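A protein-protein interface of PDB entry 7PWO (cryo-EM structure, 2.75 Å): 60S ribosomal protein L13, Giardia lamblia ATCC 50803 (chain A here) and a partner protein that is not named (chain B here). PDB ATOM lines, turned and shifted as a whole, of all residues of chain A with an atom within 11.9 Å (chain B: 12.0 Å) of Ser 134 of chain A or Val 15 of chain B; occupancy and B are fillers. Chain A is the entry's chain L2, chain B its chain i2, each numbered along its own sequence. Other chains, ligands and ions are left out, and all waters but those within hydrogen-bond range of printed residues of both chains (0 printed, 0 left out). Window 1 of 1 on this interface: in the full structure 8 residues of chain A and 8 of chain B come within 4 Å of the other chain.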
ATOM      1  N   SER A  86     -22.805 -14.776  -4.533  1.00  0.00           N
ATOM      2  CA  SER A  86     -21.505 -15.425  -4.677  1.00  0.00           C
ATOM      3  C   SER A  86     -21.107 -15.440  -6.148  1.00  0.00           C
ATOM      4  O   SER A  86     -21.857 -15.950  -6.982  1.00  0.00           O
ATOM      5  CB  SER A  86     -21.577 -16.853  -4.141  1.00  0.00           C
ATOM      6  OG  SER A  86     -20.352 -17.533  -4.291  1.00  0.00           O
ATOM      7  N   VAL A  87     -19.928 -14.898  -6.470  1.00  0.00           N
ATOM      8  CA  VAL A  87     -19.504 -14.761  -7.862  1.00  0.00           C
ATOM      9  C   VAL A  87     -18.076 -15.268  -8.023  1.00  0.00           C
ATOM     10  O   VAL A  87     -17.330 -15.417  -7.061  1.00  0.00           O
ATOM     11  CB  VAL A  87     -19.601 -13.311  -8.382  1.00  0.00           C
ATOM     12  CG1 VAL A  87     -21.047 -12.918  -8.645  1.00  0.00           C
ATOM     13  CG2 VAL A  87     -18.875 -12.336  -7.453  1.00  0.00           C
ATOM     14  N   THR A  88     -17.694 -15.491  -9.272  1.00  0.00           N
ATOM     15  CA  THR A  88     -16.384 -16.021  -9.622  1.00  0.00           C
ATOM     16  C   THR A  88     -15.430 -14.891  -9.990  1.00  0.00           C
ATOM     17  O   THR A  88     -15.784 -13.998 -10.769  1.00  0.00           O
ATOM     18  CB  THR A  88     -16.517 -17.025 -10.769  1.00  0.00           C
ATOM     19  OG1 THR A  88     -17.133 -18.216 -10.272  1.00  0.00           O
ATOM     20  CG2 THR A  88     -15.175 -17.372 -11.373  1.00  0.00           C
ATOM     21  N   ARG A  89     -14.226 -14.934  -9.423  1.00  0.00           N
ATOM     22  CA  ARG A  89     -13.218 -13.910  -9.657  1.00  0.00           C
ATOM     23  C   ARG A  89     -12.752 -13.910 -11.112  1.00  0.00           C
ATOM     24  O   ARG A  89     -12.760 -14.937 -11.793  1.00  0.00           O
ATOM     25  CB  ARG A  89     -12.038 -14.122  -8.717  1.00  0.00           C
ATOM     26  CG  ARG A  89     -12.411 -14.344  -7.263  1.00  0.00           C
ATOM     27  CD  ARG A  89     -11.193 -14.231  -6.390  1.00  0.00           C
ATOM     28  NE  ARG A  89     -11.513 -13.849  -5.024  1.00  0.00           N
ATOM     29  CZ  ARG A  89     -11.062 -14.469  -3.934  1.00  0.00           C
ATOM     30  NH1 ARG A  89     -10.255 -15.515  -4.030  1.00  0.00           N
ATOM     31  NH2 ARG A  89     -11.423 -14.030  -2.741  1.00  0.00           N
ATOM     32  N   ASN A  95      -9.424 -18.185 -10.999  1.00  0.00           N
ATOM     33  CA  ASN A  95     -10.509 -18.739 -11.798  1.00  0.00           C
ATOM     34  C   ASN A  95     -11.416 -19.651 -10.988  1.00  0.00           C
ATOM     35  O   ASN A  95     -12.625 -19.676 -11.222  1.00  0.00           O
ATOM     36  CB  ASN A  95      -9.905 -19.506 -12.978  1.00  0.00           C
ATOM     37  CG  ASN A  95     -10.929 -19.935 -13.993  1.00  0.00           C
ATOM     38  OD1 ASN A  95     -12.117 -19.693 -13.839  1.00  0.00           O
ATOM     39  ND2 ASN A  95     -10.471 -20.604 -15.030  1.00  0.00           N
ATOM     40  N   GLN A  98     -14.410 -18.244  -5.357  1.00  0.00           N
ATOM     41  CA  GLN A  98     -15.526 -17.309  -5.352  1.00  0.00           C
ATOM     42  C   GLN A  98     -15.280 -16.169  -4.371  1.00  0.00           C
ATOM     43  O   GLN A  98     -14.322 -16.163  -3.603  1.00  0.00           O
ATOM     44  CB  GLN A  98     -16.849 -18.018  -5.022  1.00  0.00           C
ATOM     45  CG  GLN A  98     -17.452 -18.863  -6.146  1.00  0.00           C
ATOM     46  CD  GLN A  98     -16.722 -20.181  -6.362  1.00  0.00           C
ATOM     47  OE1 GLN A  98     -16.253 -20.476  -7.462  1.00  0.00           O
ATOM     48  NE2 GLN A  98     -16.592 -20.966  -5.295  1.00  0.00           N
ATOM     49  N   THR A 105     -29.213 -11.410  -9.868  1.00  0.00           N
ATOM     50  CA  THR A 105     -29.824 -11.149 -11.163  1.00  0.00           C
ATOM     51  C   THR A 105     -31.330 -11.396 -11.125  1.00  0.00           C
ATOM     52  O   THR A 105     -31.856 -12.093 -10.257  1.00  0.00           O
ATOM     53  CB  THR A 105     -29.172 -12.002 -12.253  1.00  0.00           C
ATOM     54  OG1 THR A 105     -29.452 -13.387 -12.026  1.00  0.00           O
ATOM     55  CG2 THR A 105     -27.674 -11.782 -12.277  1.00  0.00           C
ATOM     56  N   LEU A 106     -32.036 -10.784 -12.077  1.00  0.00           N
ATOM     57  CA  LEU A 106     -33.474 -10.999 -12.118  1.00  0.00           C
ATOM     58  C   LEU A 106     -33.803 -12.432 -12.497  1.00  0.00           C
ATOM     59  O   LEU A 106     -34.830 -12.953 -12.074  1.00  0.00           O
ATOM     60  CB  LEU A 106     -34.147 -10.013 -13.067  1.00  0.00           C
ATOM     61  CG  LEU A 106     -34.078  -8.545 -12.637  1.00  0.00           C
ATOM     62  CD1 LEU A 106     -34.657  -7.617 -13.709  1.00  0.00           C
ATOM     63  CD2 LEU A 106     -34.730  -8.324 -11.271  1.00  0.00           C
ATOM     64  N   ARG A 107     -32.936 -13.083 -13.269  1.00  0.00           N
ATOM     65  CA  ARG A 107     -33.084 -14.506 -13.548  1.00  0.00           C
ATOM     66  C   ARG A 107     -33.021 -15.314 -12.257  1.00  0.00           C
ATOM     67  O   ARG A 107     -33.838 -16.218 -12.023  1.00  0.00           O
ATOM     68  CB  ARG A 107     -31.985 -14.923 -14.521  1.00  0.00           C
ATOM     69  CG  ARG A 107     -31.835 -16.391 -14.811  1.00  0.00           C
ATOM     70  CD  ARG A 107     -32.844 -16.844 -15.853  1.00  0.00           C
ATOM     71  NE  ARG A 107     -32.738 -18.269 -16.134  1.00  0.00           N
ATOM     72  CZ  ARG A 107     -31.946 -18.779 -17.069  1.00  0.00           C
ATOM     73  NH1 ARG A 107     -31.203 -17.978 -17.821  1.00  0.00           N
ATOM     74  NH2 ARG A 107     -31.897 -20.088 -17.262  1.00  0.00           N
ATOM     75  N   GLU A 108     -32.063 -14.978 -11.390  1.00  0.00           N
ATOM     76  CA  GLU A 108     -31.958 -15.636 -10.094  1.00  0.00           C
ATOM     77  C   GLU A 108     -33.193 -15.390  -9.238  1.00  0.00           C
ATOM     78  O   GLU A 108     -33.692 -16.317  -8.591  1.00  0.00           O
ATOM     79  CB  GLU A 108     -30.693 -15.169  -9.377  1.00  0.00           C
ATOM     80  CG  GLU A 108     -29.425 -15.861  -9.854  1.00  0.00           C
ATOM     81  CD  GLU A 108     -28.164 -15.060  -9.567  1.00  0.00           C
ATOM     82  OE1 GLU A 108     -27.165 -15.244 -10.292  1.00  0.00           O
ATOM     83  OE2 GLU A 108     -28.169 -14.250  -8.618  1.00  0.00           O
ATOM     84  N   LEU A 109     -33.706 -14.155  -9.220  1.00  0.00           N
ATOM     85  CA  LEU A 109     -34.921 -13.874  -8.456  1.00  0.00           C
ATOM     86  C   LEU A 109     -36.136 -14.601  -9.022  1.00  0.00           C
ATOM     87  O   LEU A 109     -36.977 -15.094  -8.263  1.00  0.00           O
ATOM     88  CB  LEU A 109     -35.186 -12.372  -8.383  1.00  0.00           C
ATOM     89  CG  LEU A 109     -34.175 -11.545  -7.596  1.00  0.00           C
ATOM     90  CD1 LEU A 109     -34.486 -10.079  -7.717  1.00  0.00           C
ATOM     91  CD2 LEU A 109     -34.169 -11.988  -6.137  1.00  0.00           C
ATOM     92  N   ARG A 130     -26.233  -6.900 -14.046  1.00  0.00           N
ATOM     93  CA  ARG A 130     -25.515  -8.160 -14.222  1.00  0.00           C
ATOM     94  C   ARG A 130     -26.316  -9.158 -15.051  1.00  0.00           C
ATOM     95  O   ARG A 130     -27.537  -9.262 -14.920  1.00  0.00           O
ATOM     96  CB  ARG A 130     -25.192  -8.779 -12.862  1.00  0.00           C
ATOM     97  CG  ARG A 130     -24.469 -10.112 -12.932  1.00  0.00           C
ATOM     98  CD  ARG A 130     -23.616 -10.367 -11.705  1.00  0.00           C
ATOM     99  NE  ARG A 130     -24.371 -10.902 -10.581  1.00  0.00           N
ATOM    100  CZ  ARG A 130     -24.720 -12.175 -10.430  1.00  0.00           C
ATOM    101  NH1 ARG A 130     -25.394 -12.539  -9.357  1.00  0.00           N
ATOM    102  NH2 ARG A 130     -24.397 -13.083 -11.337  1.00  0.00           N
ATOM    103  N   LYS A 131     -25.609  -9.916 -15.885  1.00  0.00           N
ATOM    104  CA  LYS A 131     -26.168 -11.025 -16.646  1.00  0.00           C
ATOM    105  C   LYS A 131     -25.378 -12.286 -16.340  1.00  0.00           C
ATOM    106  O   LYS A 131     -24.151 -12.239 -16.221  1.00  0.00           O
ATOM    107  CB  LYS A 131     -26.128 -10.758 -18.145  1.00  0.00           C
ATOM    108  CG  LYS A 131     -26.853  -9.509 -18.555  1.00  0.00           C
ATOM    109  CD  LYS A 131     -28.240  -9.475 -17.948  1.00  0.00           C
ATOM    110  CE  LYS A 131     -29.072  -8.361 -18.538  1.00  0.00           C
ATOM    111  NZ  LYS A 131     -29.476  -8.692 -19.917  1.00  0.00           N
ATOM    112  N   ASN A 132     -26.078 -13.409 -16.209  1.00  0.00           N
ATOM    113  CA  ASN A 132     -25.399 -14.665 -15.945  1.00  0.00           C
ATOM    114  C   ASN A 132     -24.633 -15.126 -17.178  1.00  0.00           C
ATOM    115  O   ASN A 132     -24.954 -14.768 -18.313  1.00  0.00           O
ATOM    116  CB  ASN A 132     -26.388 -15.743 -15.503  1.00  0.00           C
ATOM    117  CG  ASN A 132     -26.909 -15.513 -14.097  1.00  0.00           C
ATOM    118  OD1 ASN A 132     -27.886 -14.800 -13.896  1.00  0.00           O
ATOM    119  ND2 ASN A 132     -26.248 -16.113 -13.116  1.00  0.00           N
ATOM    120  N   LYS A 133     -23.593 -15.917 -16.940  1.00  0.00           N
ATOM    121  CA  LYS A 133     -22.751 -16.412 -18.011  1.00  0.00           C
ATOM    122  C   LYS A 133     -22.921 -17.904 -18.246  1.00  0.00           C
ATOM    123  O   LYS A 133     -22.393 -18.422 -19.231  1.00  0.00           O
ATOM    124  CB  LYS A 133     -21.281 -16.104 -17.700  1.00  0.00           C
ATOM    125  CG  LYS A 133     -20.984 -14.624 -17.539  1.00  0.00           C
ATOM    126  CD  LYS A 133     -21.184 -13.846 -18.819  1.00  0.00           C
ATOM    127  CE  LYS A 133     -20.725 -12.418 -18.671  1.00  0.00           C
ATOM    128  NZ  LYS A 133     -21.588 -11.628 -17.763  1.00  0.00           N
ATOM    129  N   SER A 134     -23.641 -18.600 -17.375  1.00  0.00           N
ATOM    130  CA  SER A 134     -23.831 -20.041 -17.472  1.00  0.00           C
ATOM    131  C   SER A 134     -25.020 -20.422 -16.602  1.00  0.00           C
ATOM    132  O   SER A 134     -25.677 -19.566 -16.009  1.00  0.00           O
ATOM    133  CB  SER A 134     -22.572 -20.794 -17.046  1.00  0.00           C
ATOM    134  OG  SER A 134     -22.087 -20.312 -15.809  1.00  0.00           O
ATOM    135  N   GLU A 135     -25.285 -21.722 -16.520  1.00  0.00           N
ATOM    136  CA  GLU A 135     -26.348 -22.238 -15.668  1.00  0.00           C
ATOM    137  C   GLU A 135     -25.880 -22.535 -14.247  1.00  0.00           C
ATOM    138  O   GLU A 135     -26.692 -22.491 -13.309  1.00  0.00           O
ATOM    139  CB  GLU A 135     -26.939 -23.508 -16.282  1.00  0.00           C
ATOM    140  CG  GLU A 135     -27.702 -23.298 -17.574  1.00  0.00           C
ATOM    141  CD  GLU A 135     -28.508 -22.009 -17.589  1.00  0.00           C
ATOM    142  OE1 GLU A 135     -29.576 -21.961 -16.949  1.00  0.00           O
ATOM    143  OE2 GLU A 135     -28.074 -21.040 -18.241  1.00  0.00           O
ATOM    144  N   GLU A 136     -24.589 -22.808 -14.063  1.00  0.00           N
ATOM    145  CA  GLU A 136     -24.071 -23.090 -12.729  1.00  0.00           C
ATOM    146  C   GLU A 136     -24.087 -21.846 -11.851  1.00  0.00           C
ATOM    147  O   GLU A 136     -24.347 -21.938 -10.641  1.00  0.00           O
ATOM    148  CB  GLU A 136     -22.662 -23.674 -12.834  1.00  0.00           C
ATOM    149  CG  GLU A 136     -22.599 -25.076 -13.465  1.00  0.00           C
ATOM    150  CD  GLU A 136     -22.893 -25.097 -14.964  1.00  0.00           C
ATOM    151  OE1 GLU A 136     -22.680 -26.149 -15.601  1.00  0.00           O
ATOM    152  OE2 GLU A 136     -23.315 -24.062 -15.518  1.00  0.00           O
ATOM    153  N   SER A 137     -23.801 -20.677 -12.436  1.00  0.00           N
ATOM    154  CA  SER A 137     -23.956 -19.418 -11.717  1.00  0.00           C
ATOM    155  C   SER A 137     -25.334 -19.343 -11.089  1.00  0.00           C
ATOM    156  O   SER A 137     -25.485 -19.058  -9.890  1.00  0.00           O
ATOM    157  CB  SER A 137     -23.761 -18.239 -12.672  1.00  0.00           C
ATOM    158  OG  SER A 137     -22.455 -18.188 -13.203  1.00  0.00           O
ATOM    159  N   VAL A 138     -26.351 -19.650 -11.894  1.00  0.00           N
ATOM    160  CA  VAL A 138     -27.730 -19.590 -11.438  1.00  0.00           C
ATOM    161  C   VAL A 138     -27.970 -20.596 -10.325  1.00  0.00           C
ATOM    162  O   VAL A 138     -28.573 -20.269  -9.304  1.00  0.00           O
ATOM    163  CB  VAL A 138     -28.690 -19.815 -12.612  1.00  0.00           C
ATOM    164  CG1 VAL A 138     -30.115 -19.659 -12.147  1.00  0.00           C
ATOM    165  CG2 VAL A 138     -28.363 -18.850 -13.753  1.00  0.00           C
ATOM    166  N   ALA A 139     -27.529 -21.840 -10.511  1.00  0.00           N
ATOM    167  CA  ALA A 139     -27.819 -22.855  -9.498  1.00  0.00           C
ATOM    168  C   ALA A 139     -27.218 -22.483  -8.143  1.00  0.00           C
ATOM    169  O   ALA A 139     -27.891 -22.571  -7.106  1.00  0.00           O
ATOM    170  CB  ALA A 139     -27.306 -24.217  -9.951  1.00  0.00           C
ATOM    171  N   ARG A 140     -25.962 -22.037  -8.142  1.00  0.00           N
ATOM    172  CA  ARG A 140     -25.298 -21.647  -6.904  1.00  0.00           C
ATOM    173  C   ARG A 140     -26.019 -20.479  -6.231  1.00  0.00           C
ATOM    174  O   ARG A 140     -26.290 -20.509  -5.016  1.00  0.00           O
ATOM    175  CB  ARG A 140     -23.844 -21.300  -7.217  1.00  0.00           C
ATOM    176  CG  ARG A 140     -22.889 -21.328  -6.064  1.00  0.00           C
ATOM    177  CD  ARG A 140     -21.516 -20.852  -6.504  1.00  0.00           C
ATOM    178  NE  ARG A 140     -21.584 -19.761  -7.467  1.00  0.00           N
ATOM    179  CZ  ARG A 140     -20.932 -19.749  -8.622  1.00  0.00           C
ATOM    180  NH1 ARG A 140     -20.170 -20.778  -8.960  1.00  0.00           N
ATOM    181  NH2 ARG A 140     -21.059 -18.714  -9.445  1.00  0.00           N
ATOM    182  N   ASN A 141     -26.393 -19.459  -7.010  1.00  0.00           N
ATOM    183  CA  ASN A 141     -26.999 -18.286  -6.397  1.00  0.00           C
ATOM    184  C   ASN A 141     -28.449 -18.519  -5.984  1.00  0.00           C
ATOM    185  O   ASN A 141     -28.915 -17.912  -5.017  1.00  0.00           O
ATOM    186  CB  ASN A 141     -26.913 -17.099  -7.348  1.00  0.00           C
ATOM    187  CG  ASN A 141     -25.566 -16.425  -7.313  1.00  0.00           C
ATOM    188  OD1 ASN A 141     -25.098 -16.015  -6.263  1.00  0.00           O
ATOM    189  ND2 ASN A 141     -24.944 -16.291  -8.472  1.00  0.00           N
ATOM    190  N   VAL A 142     -29.177 -19.373  -6.703  1.00  0.00           N
ATOM    191  CA  VAL A 142     -30.538 -19.713  -6.311  1.00  0.00           C
ATOM    192  C   VAL A 142     -30.524 -20.541  -5.038  1.00  0.00           C
ATOM    193  O   VAL A 142     -31.384 -20.370  -4.169  1.00  0.00           O
ATOM    194  CB  VAL A 142     -31.272 -20.423  -7.466  1.00  0.00           C
ATOM    195  CG1 VAL A 142     -32.639 -20.879  -7.043  1.00  0.00           C
ATOM    196  CG2 VAL A 142     -31.433 -19.482  -8.653  1.00  0.00           C
ATOM    197  N   LYS B   9      -9.725 -28.102 -23.990  1.00  0.00           N
ATOM    198  CA  LYS B   9     -10.903 -28.319 -23.154  1.00  0.00           C
ATOM    199  C   LYS B   9     -11.490 -27.002 -22.637  1.00  0.00           C
ATOM    200  O   LYS B   9     -12.061 -26.965 -21.548  1.00  0.00           O
ATOM    201  CB  LYS B   9     -10.588 -29.235 -21.963  1.00  0.00           C
ATOM    202  CG  LYS B   9     -10.079 -30.603 -22.328  1.00  0.00           C
ATOM    203  CD  LYS B   9     -11.078 -31.464 -23.053  1.00  0.00           C
ATOM    204  CE  LYS B   9     -10.498 -32.852 -23.205  1.00  0.00           C
ATOM    205  NZ  LYS B   9      -9.351 -32.836 -24.153  1.00  0.00           N
ATOM    206  N   LYS B  10     -11.352 -25.908 -23.384  1.00  0.00           N
ATOM    207  CA  LYS B  10     -11.922 -24.630 -22.962  1.00  0.00           C
ATOM    208  C   LYS B  10     -13.427 -24.635 -23.206  1.00  0.00           C
ATOM    209  O   LYS B  10     -13.877 -24.726 -24.355  1.00  0.00           O
ATOM    210  CB  LYS B  10     -11.267 -23.463 -23.699  1.00  0.00           C
ATOM    211  CG  LYS B  10     -11.496 -22.107 -23.032  1.00  0.00           C
ATOM    212  CD  LYS B  10     -10.885 -20.964 -23.826  1.00  0.00           C
ATOM    213  CE  LYS B  10      -9.447 -20.719 -23.416  1.00  0.00           C
ATOM    214  NZ  LYS B  10      -9.107 -19.291 -23.275  1.00  0.00           N
ATOM    215  N   GLY B  11     -14.199 -24.498 -22.132  1.00  0.00           N
ATOM    216  CA  GLY B  11     -15.634 -24.695 -22.181  1.00  0.00           C
ATOM    217  C   GLY B  11     -16.018 -26.126 -21.863  1.00  0.00           C
ATOM    218  O   GLY B  11     -16.885 -26.709 -22.520  1.00  0.00           O
ATOM    219  N   GLY B  12     -15.377 -26.705 -20.856  1.00  0.00           N
ATOM    220  CA  GLY B  12     -15.543 -28.112 -20.561  1.00  0.00           C
ATOM    221  C   GLY B  12     -16.390 -28.412 -19.347  1.00  0.00           C
ATOM    222  O   GLY B  12     -17.079 -29.435 -19.309  1.00  0.00           O
ATOM    223  N   ALA B  13     -16.363 -27.532 -18.349  1.00  0.00           N
ATOM    224  CA  ALA B  13     -17.085 -27.795 -17.111  1.00  0.00           C
ATOM    225  C   ALA B  13     -18.515 -27.265 -17.147  1.00  0.00           C
ATOM    226  O   ALA B  13     -19.451 -27.984 -16.786  1.00  0.00           O
ATOM    227  CB  ALA B  13     -16.332 -27.194 -15.920  1.00  0.00           C
ATOM    228  N   VAL B  14     -18.706 -26.037 -17.621  1.00  0.00           N
ATOM    229  CA  VAL B  14     -19.983 -25.344 -17.489  1.00  0.00           C
ATOM    230  C   VAL B  14     -20.712 -25.340 -18.826  1.00  0.00           C
ATOM    231  O   VAL B  14     -20.157 -25.743 -19.849  1.00  0.00           O
ATOM    232  CB  VAL B  14     -19.788 -23.901 -16.983  1.00  0.00           C
ATOM    233  CG1 VAL B  14     -18.961 -23.885 -15.707  1.00  0.00           C
ATOM    234  CG2 VAL B  14     -19.163 -23.021 -18.072  1.00  0.00           C
ATOM    235  N   VAL B  15     -21.967 -24.899 -18.809  1.00  0.00           N
ATOM    236  CA  VAL B  15     -22.799 -24.745 -19.997  1.00  0.00           C
ATOM    237  C   VAL B  15     -23.070 -23.258 -20.169  1.00  0.00           C
ATOM    238  O   VAL B  15     -23.689 -22.640 -19.297  1.00  0.00           O
ATOM    239  CB  VAL B  15     -24.118 -25.522 -19.870  1.00  0.00           C
ATOM    240  CG1 VAL B  15     -24.865 -25.528 -21.181  1.00  0.00           C
ATOM    241  CG2 VAL B  15     -23.855 -26.937 -19.394  1.00  0.00           C
ATOM    242  N   ARG B  16     -22.620 -22.688 -21.283  1.00  0.00           N
ATOM    243  CA  ARG B  16     -22.761 -21.253 -21.490  1.00  0.00           C
ATOM    244  C   ARG B  16     -24.209 -20.879 -21.792  1.00  0.00           C
ATOM    245  O   ARG B  16     -25.069 -21.729 -22.025  1.00  0.00           O
ATOM    246  CB  ARG B  16     -21.847 -20.763 -22.617  1.00  0.00           C
ATOM    247  CG  ARG B  16     -20.539 -20.172 -22.119  1.00  0.00           C
ATOM    248  CD  ARG B  16     -19.450 -20.107 -23.193  1.00  0.00           C
ATOM    249  NE  ARG B  16     -18.130 -19.977 -22.584  1.00  0.00           N
ATOM    250  CZ  ARG B  16     -17.362 -21.010 -22.257  1.00  0.00           C
ATOM    251  NH1 ARG B  16     -17.785 -22.244 -22.495  1.00  0.00           N
ATOM    252  NH2 ARG B  16     -16.180 -20.811 -21.687  1.00  0.00           N
ATOM    253  N   ILE B  17     -24.474 -19.575 -21.750  1.00  0.00           N
ATOM    254  CA  ILE B  17     -25.749 -18.992 -22.158  1.00  0.00           C
ATOM    255  C   ILE B  17     -25.538 -18.256 -23.473  1.00  0.00           C
ATOM    256  O   ILE B  17     -24.734 -17.319 -23.552  1.00  0.00           O
ATOM    257  CB  ILE B  17     -26.315 -18.038 -21.096  1.00  0.00           C
ATOM    258  CG1 ILE B  17     -26.629 -18.793 -19.801  1.00  0.00           C
ATOM    259  CG2 ILE B  17     -27.508 -17.249 -21.659  1.00  0.00           C
ATOM    260  CD1 ILE B  17     -26.946 -17.920 -18.630  1.00  0.00           C
ATOM    261  N   VAL B  18     -26.250 -18.683 -24.507  1.00  0.00           N
ATOM    262  CA  VAL B  18     -26.259 -17.984 -25.785  1.00  0.00           C
ATOM    263  C   VAL B  18     -27.510 -17.110 -25.780  1.00  0.00           C
ATOM    264  O   VAL B  18     -28.593 -17.512 -26.202  1.00  0.00           O
ATOM    265  CB  VAL B  18     -26.191 -18.954 -26.966  1.00  0.00           C
ATOM    266  CG1 VAL B  18     -24.786 -19.521 -27.062  1.00  0.00           C
ATOM    267  CG2 VAL B  18     -27.190 -20.101 -26.800  1.00  0.00           C
ATOM    268  N   ARG B  19     -27.349 -15.889 -25.277  1.00  0.00           N
ATOM    269  CA  ARG B  19     -28.451 -14.954 -25.136  1.00  0.00           C
ATOM    270  C   ARG B  19     -29.024 -14.551 -26.495  1.00  0.00           C
ATOM    271  O   ARG B  19     -28.392 -14.704 -27.544  1.00  0.00           O
ATOM    272  CB  ARG B  19     -27.991 -13.716 -24.367  1.00  0.00           C
ATOM    273  CG  ARG B  19     -26.634 -13.224 -24.796  1.00  0.00           C
ATOM    274  CD  ARG B  19     -25.978 -12.355 -23.727  1.00  0.00           C
ATOM    275  NE  ARG B  19     -26.503 -10.994 -23.742  1.00  0.00           N
ATOM    276  CZ  ARG B  19     -25.973  -9.985 -23.066  1.00  0.00           C
ATOM    277  NH1 ARG B  19     -24.898 -10.181 -22.311  1.00  0.00           N
ATOM    278  NH2 ARG B  19     -26.522  -8.779 -23.138  1.00  0.00           N
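Of the printed residues of chain B, Asn 132 of chain A touches Ile 17.
Of chain B, only Arg 16 and Ile 17 come within 4 Å of Lys 133 of chain A.
Of chain B, only Val 15 and Ile 17 come within 4 Å of Ser 134 of chain A.
Glu 136 of chain A touches just these residues of chain B: Ala 13, Val 14 and Val 15.
No residue of chain B comes within 4 Å of Ser 137 of chain A.
No residue of chain B comes within 4 Å of Val 138 of chain A.
Ala 139 of chain A touches none of the printed residues of chain B.
Lys 9 of chain B touches none of the printed residues of chain A.
Of chain A, only Glu 136 comes within 4 Å of Ala 13 of chain B.
Val 15 of chain B touches three residues of chain A.
Arg 16 of chain B touches one residue of chain A.
Ile 17 of chain B touches just these residues of chain A: Asn 132, Lys 133, Ser 134 and Glu 135.
The nearest residue of chain A that does not touch Val 15 of chain B is Lys 133 of chain A (4.4 Å).
Of the 24 printed residues of chain A, 5 touch a printed residue of chain B.
Of the 11 printed residues of chain B, 5 touch a printed residue of chain A.
Hydrophobic or aromatic side chains of chain B within 4 Å of the printed part of chain A: Val 14 and Ile 17.
Among the printed residues, 10 pairs touch across the chains.
O of Lys 133 of chain A lies within hydrogen-bond range of N of Ile 17 of chain B (3.5 Å).
The backbone NH of Glu 135 of chain A sits at hydrogen-bond distance from the backbone carbonyl oxygen of Val 15 of chain B, 3.3 Å away.
Among the printed residues, pairs that only touch across the chains: Asn 132 of chain A with Ile 17 of chain B, Lys 133 of chain A with Arg 16 of chain B, Ser 134 of chain A with Val 15 of chain B, Ser 134 of chain A with Ile 17 of chain B, Glu 135 of chain A with Ile 17 of chain B, Glu 136 of chain A with Ala 13 of chain B, Glu 136 of chain A with Val 14 of chain B and Glu 136 of chain A with Val 15 of chain B.
OD1 of Asn 132 of chain A sits at hydrogen-bond distance from OG1 of Thr 105 of chain A, at 2.8 Å.
NZ of Lys 133 of chain A is in hydrogen-bond range of O of Lys 131 of chain A (3.1 Å).
The guanidinium group of Arg 107 of chain A lies within salt-bridge range of the side-chain carboxylate of Glu 135 of chain A (3.0 Å).
The side-chain hydroxyl of Ser 134 of chain A sits at hydrogen-bond distance from the side-chain hydroxyl of Ser 137 of chain A (3.4 Å).
ND2 of Asn 132 of chain A lies within hydrogen-bond range of OE1 of Glu 108 of chain A (3.1 Å).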
